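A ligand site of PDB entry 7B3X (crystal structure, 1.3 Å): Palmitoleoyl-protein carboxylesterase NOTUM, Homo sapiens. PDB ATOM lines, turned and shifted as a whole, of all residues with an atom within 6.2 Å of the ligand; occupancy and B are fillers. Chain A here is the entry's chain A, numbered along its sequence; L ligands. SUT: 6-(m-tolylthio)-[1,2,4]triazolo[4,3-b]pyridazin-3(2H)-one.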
ATOM      1  N   GLY A  49     -11.932  36.704   1.588  1.00  0.00           N
ATOM      2  CA  GLY A  49     -12.461  35.647   0.755  1.00  0.00           C
ATOM      3  C   GLY A  49     -13.872  35.911   0.263  1.00  0.00           C
ATOM      4  O   GLY A  49     -14.399  37.030   0.344  1.00  0.00           O
ATOM      5  N   GLY A  50     -14.487  34.867  -0.288  1.00  0.00           N
ATOM      6  CA  GLY A  50     -15.834  34.977  -0.839  1.00  0.00           C
ATOM      7  C   GLY A  50     -16.049  34.282  -2.169  1.00  0.00           C
ATOM      8  O   GLY A  50     -16.684  34.843  -3.060  1.00  0.00           O
ATOM      9  N   TRP A  51     -15.556  33.044  -2.315  1.00  0.00           N
ATOM     10  CA  TRP A  51     -15.794  32.217  -3.516  1.00  0.00           C
ATOM     11  C   TRP A  51     -15.240  32.933  -4.752  1.00  0.00           C
ATOM     12  O   TRP A  51     -14.133  33.490  -4.686  1.00  0.00           O
ATOM     13  CB  TRP A  51     -17.219  31.729  -3.591  1.00  0.00           C
ATOM     14  CG  TRP A  51     -17.562  30.822  -2.462  1.00  0.00           C
ATOM     15  CD1 TRP A  51     -18.117  31.158  -1.273  1.00  0.00           C
ATOM     16  CD2 TRP A  51     -17.342  29.400  -2.430  1.00  0.00           C
ATOM     17  NE1 TRP A  51     -18.281  30.026  -0.494  1.00  0.00           N
ATOM     18  CE2 TRP A  51     -17.805  28.940  -1.183  1.00  0.00           C
ATOM     19  CE3 TRP A  51     -16.817  28.488  -3.336  1.00  0.00           C
ATOM     20  CZ2 TRP A  51     -17.763  27.599  -0.818  1.00  0.00           C
ATOM     21  CZ3 TRP A  51     -16.761  27.145  -2.974  1.00  0.00           C
ATOM     22  CH2 TRP A  51     -17.233  26.719  -1.722  1.00  0.00           C
ATOM     23  N   TYR A  52     -15.971  32.921  -5.877  1.00  0.00           N
ATOM     24  CA  TYR A  52     -15.481  33.420  -7.159  1.00  0.00           C
ATOM     25  C   TYR A  52     -16.649  33.289  -8.131  1.00  0.00           C
ATOM     26  O   TYR A  52     -17.703  32.746  -7.776  1.00  0.00           O
ATOM     27  CB  TYR A  52     -14.253  32.624  -7.639  1.00  0.00           C
ATOM     28  CG  TYR A  52     -14.502  31.152  -7.817  1.00  0.00           C
ATOM     29  CD1 TYR A  52     -14.265  30.264  -6.775  1.00  0.00           C
ATOM     30  CD2 TYR A  52     -14.906  30.639  -9.032  1.00  0.00           C
ATOM     31  CE1 TYR A  52     -14.481  28.898  -6.921  1.00  0.00           C
ATOM     32  CE2 TYR A  52     -15.113  29.271  -9.210  1.00  0.00           C
ATOM     33  CZ  TYR A  52     -14.906  28.413  -8.150  1.00  0.00           C
ATOM     34  OH  TYR A  52     -15.109  27.060  -8.318  1.00  0.00           O
ATOM     35  N   TYR A 105     -11.918  41.860  -1.299  1.00  0.00           N
ATOM     36  CA  TYR A 105     -11.939  40.946  -2.439  1.00  0.00           C
ATOM     37  C   TYR A 105     -13.041  41.430  -3.385  1.00  0.00           C
ATOM     38  O   TYR A 105     -14.228  41.291  -3.084  1.00  0.00           O
ATOM     39  CB  TYR A 105     -12.222  39.548  -1.907  1.00  0.00           C
ATOM     40  CG  TYR A 105     -12.312  38.438  -2.923  1.00  0.00           C
ATOM     41  CD1 TYR A 105     -11.421  38.348  -3.974  1.00  0.00           C
ATOM     42  CD2 TYR A 105     -13.247  37.414  -2.751  1.00  0.00           C
ATOM     43  CE1 TYR A 105     -11.476  37.282  -4.868  1.00  0.00           C
ATOM     44  CE2 TYR A 105     -13.305  36.356  -3.625  1.00  0.00           C
ATOM     45  CZ  TYR A 105     -12.412  36.294  -4.686  1.00  0.00           C
ATOM     46  OH  TYR A 105     -12.451  35.240  -5.573  1.00  0.00           O
ATOM     47  N   VAL A 110     -10.263  34.381  -7.105  1.00  0.00           N
ATOM     48  CA  VAL A 110      -9.401  33.752  -6.101  1.00  0.00           C
ATOM     49  C   VAL A 110      -8.048  34.470  -6.109  1.00  0.00           C
ATOM     50  O   VAL A 110      -6.990  33.866  -5.870  1.00  0.00           O
ATOM     51  CB  VAL A 110      -9.265  32.236  -6.362  1.00  0.00           C
ATOM     52  CG1 VAL A 110      -8.656  31.540  -5.149  1.00  0.00           C
ATOM     53  CG2 VAL A 110     -10.588  31.597  -6.742  1.00  0.00           C
ATOM     54  N   SER A 154      -8.187  34.554   4.250  1.00  0.00           N
ATOM     55  CA  SER A 154      -9.106  33.490   4.632  1.00  0.00           C
ATOM     56  C   SER A 154      -9.946  33.044   3.441  1.00  0.00           C
ATOM     57  O   SER A 154     -10.389  33.869   2.629  1.00  0.00           O
ATOM     58  CB  SER A 154     -10.049  33.933   5.760  1.00  0.00           C
ATOM     59  OG  SER A 154      -9.348  34.223   6.968  1.00  0.00           O
ATOM     60  N   SER A 155     -10.159  31.741   3.349  1.00  0.00           N
ATOM     61  CA  SER A 155     -11.039  31.120   2.345  1.00  0.00           C
ATOM     62  C   SER A 155     -10.439  31.362   0.962  1.00  0.00           C
ATOM     63  O   SER A 155      -9.277  31.000   0.747  1.00  0.00           O
ATOM     64  CB  SER A 155     -12.466  31.598   2.568  1.00  0.00           C
ATOM     65  OG  SER A 155     -12.957  31.141   3.820  1.00  0.00           O
ATOM     66  N   ALA A 156     -11.173  31.960   0.010  1.00  0.00           N
ATOM     67  CA  ALA A 156     -10.546  32.326  -1.262  1.00  0.00           C
ATOM     68  C   ALA A 156      -9.310  33.196  -1.053  1.00  0.00           C
ATOM     69  O   ALA A 156      -8.372  33.124  -1.845  1.00  0.00           O
ATOM     70  CB  ALA A 156     -11.545  33.026  -2.185  1.00  0.00           C
ATOM     71  N   GLY A 157      -9.315  34.026   0.000  1.00  0.00           N
ATOM     72  CA  GLY A 157      -8.120  34.787   0.341  1.00  0.00           C
ATOM     73  C   GLY A 157      -6.962  33.938   0.831  1.00  0.00           C
ATOM     74  O   GLY A 157      -5.804  34.286   0.630  1.00  0.00           O
ATOM     75  N   THR A 159      -6.362  30.750  -0.235  1.00  0.00           N
ATOM     76  CA  THR A 159      -5.783  30.285  -1.482  1.00  0.00           C
ATOM     77  C   THR A 159      -5.029  31.410  -2.188  1.00  0.00           C
ATOM     78  O   THR A 159      -3.943  31.194  -2.738  1.00  0.00           O
ATOM     79  CB  THR A 159      -6.879  29.704  -2.385  1.00  0.00           C
ATOM     80  OG1 THR A 159      -7.670  28.785  -1.623  1.00  0.00           O
ATOM     81  CG2 THR A 159      -6.263  28.998  -3.585  1.00  0.00           C
ATOM     82  N   SER A 188      -7.943  28.504   5.891  1.00  0.00           N
ATOM     83  CA  SER A 188      -9.143  27.938   5.297  1.00  0.00           C
ATOM     84  C   SER A 188      -9.098  27.986   3.767  1.00  0.00           C
ATOM     85  O   SER A 188     -10.138  28.103   3.108  1.00  0.00           O
ATOM     86  CB  SER A 188     -10.403  28.611   5.844  1.00  0.00           C
ATOM     87  OG  SER A 188     -10.461  28.436   7.261  1.00  0.00           O
ATOM     88  N   GLY A 189      -7.892  27.896   3.199  1.00  0.00           N
ATOM     89  CA  GLY A 189      -7.729  27.897   1.760  1.00  0.00           C
ATOM     90  C   GLY A 189      -7.015  26.680   1.244  1.00  0.00           C
ATOM     91  O   GLY A 189      -6.530  26.698   0.104  1.00  0.00           O
ATOM     92  N   PHE A 191      -7.536  23.053   0.196  1.00  0.00           N
ATOM     93  CA  PHE A 191      -8.631  22.172  -0.193  1.00  0.00           C
ATOM     94  C   PHE A 191      -8.100  20.909  -0.860  1.00  0.00           C
ATOM     95  O   PHE A 191      -6.959  20.867  -1.339  1.00  0.00           O
ATOM     96  CB  PHE A 191      -9.585  22.913  -1.140  1.00  0.00           C
ATOM     97  CG  PHE A 191     -10.232  24.079  -0.490  1.00  0.00           C
ATOM     98  CD1 PHE A 191     -11.088  23.898   0.582  1.00  0.00           C
ATOM     99  CD2 PHE A 191      -9.907  25.362  -0.867  1.00  0.00           C
ATOM    100  CE1 PHE A 191     -11.639  24.979   1.219  1.00  0.00           C
ATOM    101  CE2 PHE A 191     -10.466  26.452  -0.239  1.00  0.00           C
ATOM    102  CZ  PHE A 191     -11.322  26.267   0.796  1.00  0.00           C
ATOM    103  N   PRO A 210     -16.145  21.456  -9.044  1.00  0.00           N
ATOM    104  CA  PRO A 210     -15.300  22.529  -8.523  1.00  0.00           C
ATOM    105  C   PRO A 210     -14.016  22.700  -9.324  1.00  0.00           C
ATOM    106  O   PRO A 210     -13.631  23.828  -9.620  1.00  0.00           O
ATOM    107  CB  PRO A 210     -14.966  22.067  -7.096  1.00  0.00           C
ATOM    108  CG  PRO A 210     -15.949  20.973  -6.774  1.00  0.00           C
ATOM    109  CD  PRO A 210     -16.786  20.674  -7.972  1.00  0.00           C
ATOM    110  N   THR A 211     -13.354  21.590  -9.676  1.00  0.00           N
ATOM    111  CA  THR A 211     -12.164  21.688 -10.515  1.00  0.00           C
ATOM    112  C   THR A 211     -12.520  22.163 -11.911  1.00  0.00           C
ATOM    113  O   THR A 211     -11.758  22.899 -12.540  1.00  0.00           O
ATOM    114  CB  THR A 211     -11.393  20.370 -10.547  1.00  0.00           C
ATOM    115  OG1 THR A 211     -12.199  19.359 -11.182  1.00  0.00           O
ATOM    116  CG2 THR A 211     -11.024  19.920  -9.140  1.00  0.00           C
ATOM    117  N   ILE A 214     -12.988  26.055 -11.548  1.00  0.00           N
ATOM    118  CA  ILE A 214     -11.696  26.738 -11.545  1.00  0.00           C
ATOM    119  C   ILE A 214     -11.012  26.685 -12.902  1.00  0.00           C
ATOM    120  O   ILE A 214     -10.449  27.685 -13.368  1.00  0.00           O
ATOM    121  CB  ILE A 214     -10.786  26.205 -10.417  1.00  0.00           C
ATOM    122  CG1 ILE A 214     -11.409  26.503  -9.054  1.00  0.00           C
ATOM    123  CG2 ILE A 214      -9.351  26.757 -10.544  1.00  0.00           C
ATOM    124  CD1 ILE A 214     -11.576  27.995  -8.832  1.00  0.00           C
ATOM    125  N   PHE A 242      -4.142  25.657  -7.610  1.00  0.00           N
ATOM    126  CA  PHE A 242      -5.104  26.170  -6.642  1.00  0.00           C
ATOM    127  C   PHE A 242      -5.258  25.244  -5.448  1.00  0.00           C
ATOM    128  O   PHE A 242      -5.957  25.609  -4.491  1.00  0.00           O
ATOM    129  CB  PHE A 242      -6.472  26.377  -7.338  1.00  0.00           C
ATOM    130  CG  PHE A 242      -6.555  27.643  -8.142  1.00  0.00           C
ATOM    131  CD1 PHE A 242      -5.720  27.843  -9.224  1.00  0.00           C
ATOM    132  CD2 PHE A 242      -7.514  28.600  -7.847  1.00  0.00           C
ATOM    133  CE1 PHE A 242      -5.799  29.013  -9.971  1.00  0.00           C
ATOM    134  CE2 PHE A 242      -7.604  29.754  -8.609  1.00  0.00           C
ATOM    135  CZ  PHE A 242      -6.745  29.962  -9.638  1.00  0.00           C
ATOM    136  N   PHE A 243      -4.642  24.072  -5.484  1.00  0.00           N
ATOM    137  CA  PHE A 243      -4.760  23.116  -4.395  1.00  0.00           C
ATOM    138  C   PHE A 243      -3.506  23.168  -3.536  1.00  0.00           C
ATOM    139  O   PHE A 243      -2.408  22.894  -4.014  1.00  0.00           O
ATOM    140  CB  PHE A 243      -5.079  21.730  -4.956  1.00  0.00           C
ATOM    141  CG  PHE A 243      -6.481  21.660  -5.484  1.00  0.00           C
ATOM    142  CD1 PHE A 243      -7.530  21.343  -4.636  1.00  0.00           C
ATOM    143  CD2 PHE A 243      -6.761  22.028  -6.782  1.00  0.00           C
ATOM    144  CE1 PHE A 243      -8.837  21.348  -5.090  1.00  0.00           C
ATOM    145  CE2 PHE A 243      -8.063  22.030  -7.243  1.00  0.00           C
ATOM    146  CZ  PHE A 243      -9.107  21.691  -6.396  1.00  0.00           C
ATOM    147  N   ASP A 263     -13.404  21.152   7.116  1.00  0.00           N
ATOM    148  CA  ASP A 263     -13.812  22.494   6.723  1.00  0.00           C
ATOM    149  C   ASP A 263     -15.189  22.442   6.075  1.00  0.00           C
ATOM    150  O   ASP A 263     -15.455  21.597   5.225  1.00  0.00           O
ATOM    151  CB  ASP A 263     -12.768  23.047   5.761  1.00  0.00           C
ATOM    152  CG  ASP A 263     -13.074  24.426   5.310  1.00  0.00           C
ATOM    153  OD1 ASP A 263     -12.641  25.374   6.004  1.00  0.00           O
ATOM    154  OD2 ASP A 263     -13.752  24.550   4.271  1.00  0.00           O
ATOM    155  N   ALA A 265     -16.605  24.392   3.936  1.00  0.00           N
ATOM    156  CA  ALA A 265     -16.647  24.617   2.492  1.00  0.00           C
ATOM    157  C   ALA A 265     -16.172  23.378   1.737  1.00  0.00           C
ATOM    158  O   ALA A 265     -16.706  23.076   0.665  1.00  0.00           O
ATOM    159  CB  ALA A 265     -15.814  25.851   2.122  1.00  0.00           C
ATOM    160  N   GLN A 266     -15.191  22.657   2.280  1.00  0.00           N
ATOM    161  CA  GLN A 266     -14.791  21.374   1.710  1.00  0.00           C
ATOM    162  C   GLN A 266     -15.952  20.398   1.714  1.00  0.00           C
ATOM    163  O   GLN A 266     -16.250  19.743   0.710  1.00  0.00           O
ATOM    164  CB  GLN A 266     -13.616  20.810   2.507  1.00  0.00           C
ATOM    165  CG  GLN A 266     -13.146  19.447   2.020  1.00  0.00           C
ATOM    166  CD  GLN A 266     -12.281  19.541   0.770  1.00  0.00           C
ATOM    167  OE1 GLN A 266     -11.320  20.310   0.722  1.00  0.00           O
ATOM    168  NE2 GLN A 266     -12.646  18.778  -0.249  1.00  0.00           N
ATOM    169  N   VAL A 269     -18.635  21.454  -1.048  1.00  0.00           N
ATOM    170  CA  VAL A 269     -18.295  21.008  -2.396  1.00  0.00           C
ATOM    171  C   VAL A 269     -18.342  19.487  -2.500  1.00  0.00           C
ATOM    172  O   VAL A 269     -18.645  18.939  -3.564  1.00  0.00           O
ATOM    173  CB  VAL A 269     -16.971  21.615  -2.909  1.00  0.00           C
ATOM    174  CG1 VAL A 269     -17.004  23.138  -2.812  1.00  0.00           C
ATOM    175  CG2 VAL A 269     -15.761  21.024  -2.178  1.00  0.00           C
ATOM    176  N   HIS A 312     -15.298  26.888   9.742  1.00  0.00           N
ATOM    177  CA  HIS A 312     -14.922  27.608   8.520  1.00  0.00           C
ATOM    178  C   HIS A 312     -14.300  28.933   8.907  1.00  0.00           C
ATOM    179  O   HIS A 312     -14.950  29.737   9.588  1.00  0.00           O
ATOM    180  CB  HIS A 312     -16.165  27.868   7.670  1.00  0.00           C
ATOM    181  CG  HIS A 312     -15.847  28.499   6.340  1.00  0.00           C
ATOM    182  ND1 HIS A 312     -14.866  28.022   5.500  1.00  0.00           N
ATOM    183  CD2 HIS A 312     -16.340  29.612   5.749  1.00  0.00           C
ATOM    184  CE1 HIS A 312     -14.798  28.794   4.426  1.00  0.00           C
ATOM    185  NE2 HIS A 312     -15.680  29.772   4.559  1.00  0.00           N
ATOM    186  N   GLU A 313     -13.083  29.180   8.415  1.00  0.00           N
ATOM    187  CA  GLU A 313     -12.284  30.375   8.710  1.00  0.00           C
ATOM    188  C   GLU A 313     -11.937  30.456  10.193  1.00  0.00           C
ATOM    189  O   GLU A 313     -12.607  29.841  11.019  1.00  0.00           O
ATOM    190  CB  GLU A 313     -12.937  31.676   8.225  1.00  0.00           C
ATOM    191  CG  GLU A 313     -13.160  31.715   6.742  1.00  0.00           C
ATOM    192  CD  GLU A 313     -13.820  33.000   6.271  1.00  0.00           C
ATOM    193  OE1 GLU A 313     -13.881  33.232   5.043  1.00  0.00           O
ATOM    194  OE2 GLU A 313     -14.260  33.786   7.136  1.00  0.00           O
HETATM  195  C01 SUT L   1     -11.590  24.400  -6.344  1.00  0.00           C
HETATM  196  C02 SUT L   1     -10.979  25.515  -5.489  1.00  0.00           C
HETATM  197  C03 SUT L   1      -9.701  25.346  -4.963  1.00  0.00           C
HETATM  198  C04 SUT L   1      -9.126  26.328  -4.182  1.00  0.00           C
HETATM  199  C05 SUT L   1      -9.823  27.498  -3.906  1.00  0.00           C
HETATM  200  C06 SUT L   1     -11.089  27.670  -4.451  1.00  0.00           C
HETATM  201  C07 SUT L   1     -11.672  26.686  -5.236  1.00  0.00           C
HETATM  202  C09 SUT L   1     -12.906  28.876  -2.617  1.00  0.00           C
HETATM  203  C12 SUT L   1     -14.507  30.818   0.026  1.00  0.00           C
HETATM  204  C16 SUT L   1     -14.379  28.560  -0.335  1.00  0.00           C
HETATM  205  C17 SUT L   1     -13.988  27.426  -1.026  1.00  0.00           C
HETATM  206  C18 SUT L   1     -13.239  27.571  -2.184  1.00  0.00           C
HETATM  207  N10 SUT L   1     -13.272  29.947  -1.947  1.00  0.00           N
HETATM  208  N11 SUT L   1     -14.009  29.779  -0.822  1.00  0.00           N
HETATM  209  N14 SUT L   1     -15.214  30.210   1.096  1.00  0.00           N
HETATM  210  N15 SUT L   1     -15.144  28.830   0.900  1.00  0.00           N
HETATM  211  O13 SUT L   1     -14.295  31.966  -0.156  1.00  0.00           O
HETATM  212  S08 SUT L   1     -11.955  29.213  -4.087  1.00  0.00           S
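An oxygen (O13) of the ligand is in hydrogen-bond range of the backbone NH (N) of Trp 51, 2.7 Å away.
The backbone NH (N) of Gly 50 lies within hydrogen-bond range of an oxygen (O13) of the ligand (2.9 Å).
The backbone NH of Ala 156 lies within hydrogen-bond range of an oxygen (O13) of the ligand (3.1 Å).
O of Trp 51 lies within hydrogen-bond range of OH of Tyr 105.
The backbone NH (N) of Ala 265 sits at hydrogen-bond distance from the side-chain carboxylate (OD2) of Asp 263.
OG of Ser 155 sits close to NE2 of His 312 (3.1 Å).
The side-chain hydroxyl (OG) of Ser 155 is in hydrogen-bond range of the side-chain carboxylate (OE1) of Glu 313 (2.6 Å).
The side-chain hydroxyl (OG1) of Thr 159 sits at hydrogen-bond distance from the backbone carbonyl oxygen (O) of Gly 189 (2.9 Å).
A ring nitrogen (ND1) of His 312 sits at hydrogen-bond distance from the side-chain carboxylate (OD1) of Asp 263 (3.5 Å).
The backbone NH (N) of Val 110 sits at hydrogen-bond distance from the side-chain hydroxyl (OH) of Tyr 105 (2.8 Å).
The backbone NH of Gly 49 lies close to the backbone carbonyl oxygen of Ser 154 (3.4 Å).
Merely in contact with the ligand: Gly 49, Tyr 52, Val 110, Ser 155, Thr 159, Phe 191, Pro 210, Ile 214, Phe 242, Phe 243, Ala 265 and His 312.
Hydrophobic or aromatic side chains within 4 Å of the ligand: Trp 51, Tyr 52, Val 110, Ala 156, Phe 191, Ile 214, Phe 243, Ala 265 and His 312.
15 residues have an atom within 4 Å of the ligand: Gly 49, Gly 50, Trp 51, Tyr 52, Val 110, Ser 155, Ala 156, Thr 159, Phe 191, Pro 210, Ile 214, Phe 242, Phe 243, Ala 265 and His 312.
The nearest printed residue that does not touch the ligand is Thr 211 (4.7 Å).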
